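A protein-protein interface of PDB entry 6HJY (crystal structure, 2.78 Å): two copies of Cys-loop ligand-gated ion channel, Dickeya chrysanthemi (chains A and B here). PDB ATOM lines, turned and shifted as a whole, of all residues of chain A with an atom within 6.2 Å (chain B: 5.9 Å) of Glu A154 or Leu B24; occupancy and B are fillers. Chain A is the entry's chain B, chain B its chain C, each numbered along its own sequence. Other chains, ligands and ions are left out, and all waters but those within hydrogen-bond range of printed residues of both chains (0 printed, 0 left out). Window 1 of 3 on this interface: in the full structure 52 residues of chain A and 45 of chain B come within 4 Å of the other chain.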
ATOM      1  N   TYR A  19      27.071   7.839  10.642  1.00  0.00           N
ATOM      2  CA  TYR A  19      27.349   8.601  11.855  1.00  0.00           C
ATOM      3  C   TYR A  19      28.808   9.057  11.886  1.00  0.00           C
ATOM      4  O   TYR A  19      29.527   8.875  10.909  1.00  0.00           O
ATOM      5  CB  TYR A  19      27.025   7.717  13.089  1.00  0.00           C
ATOM      6  CG  TYR A  19      28.025   6.599  13.333  1.00  0.00           C
ATOM      7  CD1 TYR A  19      28.024   5.450  12.540  1.00  0.00           C
ATOM      8  CD2 TYR A  19      28.946   6.671  14.373  1.00  0.00           C
ATOM      9  CE1 TYR A  19      28.944   4.422  12.758  1.00  0.00           C
ATOM     10  CE2 TYR A  19      29.876   5.656  14.592  1.00  0.00           C
ATOM     11  CZ  TYR A  19      29.869   4.532  13.783  1.00  0.00           C
ATOM     12  OH  TYR A  19      30.796   3.548  14.003  1.00  0.00           O
ATOM     13  N   GLY A  20      29.210   9.645  13.010  1.00  0.00           N
ATOM     14  CA  GLY A  20      30.570  10.104  13.273  1.00  0.00           C
ATOM     15  C   GLY A  20      31.167  11.029  12.238  1.00  0.00           C
ATOM     16  O   GLY A  20      32.334  10.855  11.880  1.00  0.00           O
ATOM     17  N   VAL A  21      30.374  12.014  11.755  1.00  0.00           N
ATOM     18  CA  VAL A  21      30.816  13.010  10.770  1.00  0.00           C
ATOM     19  C   VAL A  21      31.948  13.849  11.373  1.00  0.00           C
ATOM     20  O   VAL A  21      31.812  14.360  12.485  1.00  0.00           O
ATOM     21  CB  VAL A  21      29.651  13.900  10.228  1.00  0.00           C
ATOM     22  CG1 VAL A  21      30.167  15.023   9.329  1.00  0.00           C
ATOM     23  CG2 VAL A  21      28.613  13.068   9.482  1.00  0.00           C
ATOM     24  N   GLU A 150      12.955  10.529  13.801  1.00  0.00           N
ATOM     25  CA  GLU A 150      14.166  11.263  13.428  1.00  0.00           C
ATOM     26  C   GLU A 150      14.504  12.417  14.392  1.00  0.00           C
ATOM     27  O   GLU A 150      15.605  12.967  14.310  1.00  0.00           O
ATOM     28  CB  GLU A 150      14.081  11.749  11.969  1.00  0.00           C
ATOM     29  CG  GLU A 150      12.885  12.644  11.665  1.00  0.00           C
ATOM     30  CD  GLU A 150      12.931  13.388  10.340  1.00  0.00           C
ATOM     31  OE1 GLU A 150      13.411  12.817   9.334  1.00  0.00           O
ATOM     32  OE2 GLU A 150      12.447  14.542  10.299  1.00  0.00           O
ATOM     33  N   GLU A 151      13.558  12.767  15.305  1.00  0.00           N
ATOM     34  CA  GLU A 151      13.690  13.821  16.326  1.00  0.00           C
ATOM     35  C   GLU A 151      14.946  13.599  17.171  1.00  0.00           C
ATOM     36  O   GLU A 151      15.672  14.552  17.454  1.00  0.00           O
ATOM     37  CB  GLU A 151      12.472  13.824  17.267  1.00  0.00           C
ATOM     38  CG  GLU A 151      11.260  14.593  16.770  1.00  0.00           C
ATOM     39  CD  GLU A 151      10.144  14.681  17.800  1.00  0.00           C
ATOM     40  OE1 GLU A 151       9.598  13.621  18.183  1.00  0.00           O
ATOM     41  OE2 GLU A 151       9.829  15.808  18.245  1.00  0.00           O
ATOM     42  N   ILE A 152      15.197  12.327  17.554  1.00  0.00           N
ATOM     43  CA  ILE A 152      16.328  11.885  18.376  1.00  0.00           C
ATOM     44  C   ILE A 152      17.625  11.710  17.553  1.00  0.00           C
ATOM     45  O   ILE A 152      18.676  11.433  18.135  1.00  0.00           O
ATOM     46  CB  ILE A 152      15.975  10.609  19.216  1.00  0.00           C
ATOM     47  CG1 ILE A 152      15.948   9.319  18.358  1.00  0.00           C
ATOM     48  CG2 ILE A 152      14.668  10.799  20.009  1.00  0.00           C
ATOM     49  CD1 ILE A 152      16.460   8.053  19.053  1.00  0.00           C
ATOM     50  N   ASP A 153      17.546  11.857  16.210  1.00  0.00           N
ATOM     51  CA  ASP A 153      18.683  11.698  15.295  1.00  0.00           C
ATOM     52  C   ASP A 153      19.327  13.017  14.861  1.00  0.00           C
ATOM     53  O   ASP A 153      18.633  14.019  14.673  1.00  0.00           O
ATOM     54  CB  ASP A 153      18.279  10.877  14.056  1.00  0.00           C
ATOM     55  CG  ASP A 153      17.825   9.461  14.350  1.00  0.00           C
ATOM     56  OD1 ASP A 153      18.477   8.788  15.179  1.00  0.00           O
ATOM     57  OD2 ASP A 153      16.851   9.009  13.716  1.00  0.00           O
ATOM     58  N   GLU A 154      20.660  12.984  14.659  1.00  0.00           N
ATOM     59  CA  GLU A 154      21.484  14.116  14.234  1.00  0.00           C
ATOM     60  C   GLU A 154      21.212  14.491  12.778  1.00  0.00           C
ATOM     61  O   GLU A 154      21.204  15.678  12.438  1.00  0.00           O
ATOM     62  CB  GLU A 154      22.976  13.797  14.444  1.00  0.00           C
ATOM     63  CG  GLU A 154      23.894  15.010  14.349  1.00  0.00           C
ATOM     64  CD  GLU A 154      25.385  14.756  14.522  1.00  0.00           C
ATOM     65  OE1 GLU A 154      25.779  13.599  14.800  1.00  0.00           O
ATOM     66  OE2 GLU A 154      26.164  15.727  14.388  1.00  0.00           O
ATOM     67  N   TRP A 155      21.009  13.473  11.925  1.00  0.00           N
ATOM     68  CA  TRP A 155      20.747  13.641  10.497  1.00  0.00           C
ATOM     69  C   TRP A 155      19.367  13.146  10.096  1.00  0.00           C
ATOM     70  O   TRP A 155      18.863  12.168  10.658  1.00  0.00           O
ATOM     71  CB  TRP A 155      21.839  12.957   9.658  1.00  0.00           C
ATOM     72  CG  TRP A 155      23.167  13.645   9.765  1.00  0.00           C
ATOM     73  CD1 TRP A 155      24.197  13.313  10.595  1.00  0.00           C
ATOM     74  CD2 TRP A 155      23.576  14.830   9.068  1.00  0.00           C
ATOM     75  NE1 TRP A 155      25.237  14.202  10.439  1.00  0.00           N
ATOM     76  CE2 TRP A 155      24.883  15.146   9.509  1.00  0.00           C
ATOM     77  CE3 TRP A 155      22.975  15.643   8.094  1.00  0.00           C
ATOM     78  CZ2 TRP A 155      25.597  16.244   9.006  1.00  0.00           C
ATOM     79  CZ3 TRP A 155      23.676  16.735   7.608  1.00  0.00           C
ATOM     80  CH2 TRP A 155      24.965  17.036   8.073  1.00  0.00           C
ATOM     81  N   TRP A 156      18.756  13.837   9.123  1.00  0.00           N
ATOM     82  CA  TRP A 156      17.437  13.499   8.605  1.00  0.00           C
ATOM     83  C   TRP A 156      17.535  13.105   7.136  1.00  0.00           C
ATOM     84  O   TRP A 156      17.696  13.971   6.272  1.00  0.00           O
ATOM     85  CB  TRP A 156      16.455  14.668   8.795  1.00  0.00           C
ATOM     86  CG  TRP A 156      16.176  15.075  10.220  1.00  0.00           C
ATOM     87  CD1 TRP A 156      16.355  14.327  11.349  1.00  0.00           C
ATOM     88  CD2 TRP A 156      15.602  16.318  10.650  1.00  0.00           C
ATOM     89  NE1 TRP A 156      15.966  15.043  12.461  1.00  0.00           N
ATOM     90  CE2 TRP A 156      15.486  16.264  12.058  1.00  0.00           C
ATOM     91  CE3 TRP A 156      15.177  17.480   9.978  1.00  0.00           C
ATOM     92  CZ2 TRP A 156      14.949  17.322  12.805  1.00  0.00           C
ATOM     93  CZ3 TRP A 156      14.665  18.533  10.721  1.00  0.00           C
ATOM     94  CH2 TRP A 156      14.568  18.456  12.117  1.00  0.00           C
ATOM     95  N   VAL A 193      19.631  16.006   5.669  1.00  0.00           N
ATOM     96  CA  VAL A 193      19.541  17.393   6.147  1.00  0.00           C
ATOM     97  C   VAL A 193      19.853  17.346   7.648  1.00  0.00           C
ATOM     98  O   VAL A 193      19.374  16.437   8.333  1.00  0.00           O
ATOM     99  CB  VAL A 193      18.129  17.995   5.875  1.00  0.00           C
ATOM    100  CG1 VAL A 193      17.996  19.408   6.448  1.00  0.00           C
ATOM    101  CG2 VAL A 193      17.805  17.998   4.383  1.00  0.00           C
ATOM    102  N   ARG A 194      20.663  18.296   8.159  1.00  0.00           N
ATOM    103  CA  ARG A 194      20.992  18.319   9.584  1.00  0.00           C
ATOM    104  C   ARG A 194      19.789  18.714  10.427  1.00  0.00           C
ATOM    105  O   ARG A 194      18.947  19.489   9.969  1.00  0.00           O
ATOM    106  CB  ARG A 194      22.169  19.262   9.872  1.00  0.00           C
ATOM    107  CG  ARG A 194      22.833  19.001  11.230  1.00  0.00           C
ATOM    108  CD  ARG A 194      23.879  20.040  11.574  1.00  0.00           C
ATOM    109  NE  ARG A 194      24.980  20.031  10.609  1.00  0.00           N
ATOM    110  CZ  ARG A 194      26.065  19.265  10.694  1.00  0.00           C
ATOM    111  NH1 ARG A 194      26.214  18.424  11.712  1.00  0.00           N
ATOM    112  NH2 ARG A 194      27.007  19.335   9.766  1.00  0.00           N
ATOM    113  N   ASN A 195      19.703  18.146  11.648  1.00  0.00           N
ATOM    114  CA  ASN A 195      18.684  18.450  12.648  1.00  0.00           C
ATOM    115  C   ASN A 195      19.164  19.754  13.317  1.00  0.00           C
ATOM    116  O   ASN A 195      20.171  19.731  14.034  1.00  0.00           O
ATOM    117  CB  ASN A 195      18.582  17.287  13.665  1.00  0.00           C
ATOM    118  CG  ASN A 195      17.576  17.440  14.790  1.00  0.00           C
ATOM    119  OD1 ASN A 195      16.997  18.501  15.025  1.00  0.00           O
ATOM    120  ND2 ASN A 195      17.320  16.351  15.497  1.00  0.00           N
ATOM    121  N   PRO A 196      18.517  20.914  13.043  1.00  0.00           N
ATOM    122  CA  PRO A 196      19.016  22.171  13.615  1.00  0.00           C
ATOM    123  C   PRO A 196      18.407  22.583  14.962  1.00  0.00           C
ATOM    124  O   PRO A 196      18.715  23.675  15.440  1.00  0.00           O
ATOM    125  CB  PRO A 196      18.704  23.184  12.510  1.00  0.00           C
ATOM    126  CG  PRO A 196      17.508  22.611  11.783  1.00  0.00           C
ATOM    127  CD  PRO A 196      17.343  21.160  12.180  1.00  0.00           C
ATOM    128  N   TYR A 199      20.833  23.813  17.770  1.00  0.00           N
ATOM    129  CA  TYR A 199      21.462  25.088  17.423  1.00  0.00           C
ATOM    130  C   TYR A 199      20.481  26.258  17.338  1.00  0.00           C
ATOM    131  O   TYR A 199      20.893  27.403  17.534  1.00  0.00           O
ATOM    132  CB  TYR A 199      22.295  24.945  16.141  1.00  0.00           C
ATOM    133  CG  TYR A 199      23.353  23.863  16.251  1.00  0.00           C
ATOM    134  CD1 TYR A 199      24.551  24.099  16.921  1.00  0.00           C
ATOM    135  CD2 TYR A 199      23.135  22.591  15.732  1.00  0.00           C
ATOM    136  CE1 TYR A 199      25.505  23.093  17.073  1.00  0.00           C
ATOM    137  CE2 TYR A 199      24.092  21.583  15.859  1.00  0.00           C
ATOM    138  CZ  TYR A 199      25.273  21.839  16.535  1.00  0.00           C
ATOM    139  OH  TYR A 199      26.218  20.850  16.662  1.00  0.00           O
ATOM    140  N   ASN B  22      28.381   6.696  24.580  1.00  0.00           N
ATOM    141  CA  ASN B  22      28.680   7.803  23.689  1.00  0.00           C
ATOM    142  C   ASN B  22      27.328   8.270  23.187  1.00  0.00           C
ATOM    143  O   ASN B  22      26.740   7.640  22.301  1.00  0.00           O
ATOM    144  CB  ASN B  22      29.591   7.367  22.535  1.00  0.00           C
ATOM    145  CG  ASN B  22      30.012   8.488  21.608  1.00  0.00           C
ATOM    146  OD1 ASN B  22      29.217   9.341  21.199  1.00  0.00           O
ATOM    147  ND2 ASN B  22      31.268   8.473  21.202  1.00  0.00           N
ATOM    148  N   THR B  23      26.821   9.354  23.805  1.00  0.00           N
ATOM    149  CA  THR B  23      25.518   9.977  23.552  1.00  0.00           C
ATOM    150  C   THR B  23      25.279  10.354  22.092  1.00  0.00           C
ATOM    151  O   THR B  23      24.200  10.075  21.563  1.00  0.00           O
ATOM    152  CB  THR B  23      25.315  11.200  24.451  1.00  0.00           C
ATOM    153  OG1 THR B  23      26.429  12.079  24.296  1.00  0.00           O
ATOM    154  CG2 THR B  23      25.114  10.832  25.913  1.00  0.00           C
ATOM    155  N   LEU B  24      26.277  10.989  21.447  1.00  0.00           N
ATOM    156  CA  LEU B  24      26.150  11.430  20.060  1.00  0.00           C
ATOM    157  C   LEU B  24      26.157  10.274  19.063  1.00  0.00           C
ATOM    158  O   LEU B  24      25.410  10.317  18.083  1.00  0.00           O
ATOM    159  CB  LEU B  24      27.202  12.500  19.708  1.00  0.00           C
ATOM    160  CG  LEU B  24      26.906  13.398  18.489  1.00  0.00           C
ATOM    161  CD1 LEU B  24      25.476  13.944  18.506  1.00  0.00           C
ATOM    162  CD2 LEU B  24      27.892  14.544  18.411  1.00  0.00           C
ATOM    163  N   GLU B  25      26.972   9.229  19.326  1.00  0.00           N
ATOM    164  CA  GLU B  25      27.056   8.040  18.470  1.00  0.00           C
ATOM    165  C   GLU B  25      25.979   7.003  18.796  1.00  0.00           C
ATOM    166  O   GLU B  25      25.770   6.083  18.001  1.00  0.00           O
ATOM    167  CB  GLU B  25      28.445   7.389  18.561  1.00  0.00           C
ATOM    168  CG  GLU B  25      29.541   8.128  17.804  1.00  0.00           C
ATOM    169  CD  GLU B  25      30.875   7.404  17.684  1.00  0.00           C
ATOM    170  OE1 GLU B  25      31.039   6.323  18.299  1.00  0.00           O
ATOM    171  OE2 GLU B  25      31.766   7.928  16.976  1.00  0.00           O
ATOM    172  N   GLN B  26      25.297   7.156  19.962  1.00  0.00           N
ATOM    173  CA  GLN B  26      24.261   6.247  20.486  1.00  0.00           C
ATOM    174  C   GLN B  26      24.817   4.816  20.623  1.00  0.00           C
ATOM    175  O   GLN B  26      24.222   3.844  20.146  1.00  0.00           O
ATOM    176  CB  GLN B  26      22.958   6.309  19.660  1.00  0.00           C
ATOM    177  CG  GLN B  26      22.038   7.459  20.050  1.00  0.00           C
ATOM    178  CD  GLN B  26      20.872   7.553  19.107  1.00  0.00           C
ATOM    179  OE1 GLN B  26      19.853   6.884  19.272  1.00  0.00           O
ATOM    180  NE2 GLN B  26      21.007   8.373  18.078  1.00  0.00           N
ATOM    181  N   PHE B 111      18.114  10.864  25.071  1.00  0.00           N
ATOM    182  CA  PHE B 111      18.669  11.595  26.208  1.00  0.00           C
ATOM    183  C   PHE B 111      17.967  12.933  26.462  1.00  0.00           C
ATOM    184  O   PHE B 111      18.535  13.788  27.141  1.00  0.00           O
ATOM    185  CB  PHE B 111      20.182  11.814  26.009  1.00  0.00           C
ATOM    186  CG  PHE B 111      20.996  10.569  25.745  1.00  0.00           C
ATOM    187  CD1 PHE B 111      21.452   9.780  26.794  1.00  0.00           C
ATOM    188  CD2 PHE B 111      21.336  10.205  24.449  1.00  0.00           C
ATOM    189  CE1 PHE B 111      22.217   8.636  26.547  1.00  0.00           C
ATOM    190  CE2 PHE B 111      22.112   9.072  24.204  1.00  0.00           C
ATOM    191  CZ  PHE B 111      22.548   8.294  25.256  1.00  0.00           C
ATOM    192  N   ARG B 250      27.442  15.789  24.304  1.00  0.00           N
ATOM    193  CA  ARG B 250      27.089  16.340  22.995  1.00  0.00           C
ATOM    194  C   ARG B 250      25.836  15.662  22.451  1.00  0.00           C
ATOM    195  O   ARG B 250      25.788  14.429  22.372  1.00  0.00           O
ATOM    196  CB  ARG B 250      28.259  16.228  22.000  1.00  0.00           C
ATOM    197  CG  ARG B 250      29.332  17.315  22.160  1.00  0.00           C
ATOM    198  CD  ARG B 250      28.829  18.758  22.009  1.00  0.00           C
ATOM    199  NE  ARG B 250      28.028  18.967  20.799  1.00  0.00           N
ATOM    200  CZ  ARG B 250      26.737  19.289  20.788  1.00  0.00           C
ATOM    201  NH1 ARG B 250      26.074  19.452  21.928  1.00  0.00           N
ATOM    202  NH2 ARG B 250      26.100  19.466  19.638  1.00  0.00           N
ATOM    203  N   LEU B 251      24.805  16.467  22.121  1.00  0.00           N
ATOM    204  CA  LEU B 251      23.517  15.967  21.635  1.00  0.00           C
ATOM    205  C   LEU B 251      22.912  16.807  20.496  1.00  0.00           C
ATOM    206  O   LEU B 251      23.145  18.017  20.444  1.00  0.00           O
ATOM    207  CB  LEU B 251      22.524  15.868  22.809  1.00  0.00           C
ATOM    208  CG  LEU B 251      22.759  14.741  23.815  1.00  0.00           C
ATOM    209  CD1 LEU B 251      22.027  15.006  25.092  1.00  0.00           C
ATOM    210  CD2 LEU B 251      22.356  13.391  23.241  1.00  0.00           C
ATOM    211  N   PRO B 252      22.089  16.202  19.601  1.00  0.00           N
ATOM    212  CA  PRO B 252      21.478  16.994  18.517  1.00  0.00           C
ATOM    213  C   PRO B 252      20.148  17.666  18.902  1.00  0.00           C
ATOM    214  O   PRO B 252      19.460  18.210  18.040  1.00  0.00           O
ATOM    215  CB  PRO B 252      21.280  15.952  17.418  1.00  0.00           C
ATOM    216  CG  PRO B 252      21.026  14.679  18.155  1.00  0.00           C
ATOM    217  CD  PRO B 252      21.685  14.782  19.513  1.00  0.00           C
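The guanidinium group (NH2) of Arg B250 lies within hydrogen-bond range of the side-chain hydroxyl (OH) of Tyr A199, at 3.3 Å.
O of Glu A151 sits at hydrogen-bond distance from ND2 of Asn A195.
The backbone carbonyl oxygen of Asp A153 lies within hydrogen-bond range of the side-chain amide nitrogen of Asn A195 (2.8 Å).
The side-chain carboxylate (OE2) of Glu A154 lies within salt-bridge range of the guanidinium group (NH1) of Arg A194, 3.8 Å away.
O of Glu A154 is in hydrogen-bond range of N of Asn A195.
OD1 of Asn B22 lies within hydrogen-bond range of N of Leu B24 (3.4 Å).
OD1 of Asn B22 is in hydrogen-bond range of N of Glu B25, at 2.9 Å.
Among the printed residues, pairs that only touch across the chains: Tyr A19 with Glu B25 (3.7 Å), Ile A152 with Gln B26 (3.6 Å), Asp A153 with Gln B26 (3.9 Å), Glu A154 with Leu B24 (3.7 Å), Glu A154 with Pro B252 (3.7 Å) and Asn A195 with Pro B252 (3.8 Å).
Of the printed residues of chain B, Tyr A19 touches Glu B25 (3.7 Å).
Of chain B, only Leu B24 and Pro B252 come within 4 Å of Glu A154.
Of the printed residues of chain B, Asn A195 touches Pro B252.
Printed residues of chain B within 4 Å of Tyr A199: Arg B250 (3.3 Å).
Of the printed residues of chain A, Leu B24 touches Glu A154 (3.7 Å).
Of the printed residues of chain A, Glu B25 touches Tyr A19.
Of the printed residues of chain A, Pro B252 touches Glu A154 (3.7 Å) and Asn A195 (3.8 Å).
The nearest residue of chain A that does not touch Leu B24 is Tyr A19 (5.9 Å).
The nearest printed residue of chain A that does not touch Arg B250 is Glu A154 (6.4 Å).
Of the 15 printed residues of chain A, 6 touch a printed residue of chain B.
Hydrophobic or aromatic side chains of chain A within 4 Å of the printed part of chain B: Tyr A19, Ile A152 and Tyr A199.
Of the 9 printed residues of chain B, 5 touch a printed residue of chain A.
Hydrophobic or aromatic side chains of chain B within 4 Å of the printed part of chain A: Leu B24 and Pro B252.
Among the printed residues, 7 pairs touch across the chains.
No position is printed for both chains.
Of the 7 pairs that touch across the chains among the printed residues, none has its exchanged pair printed and touching as well.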
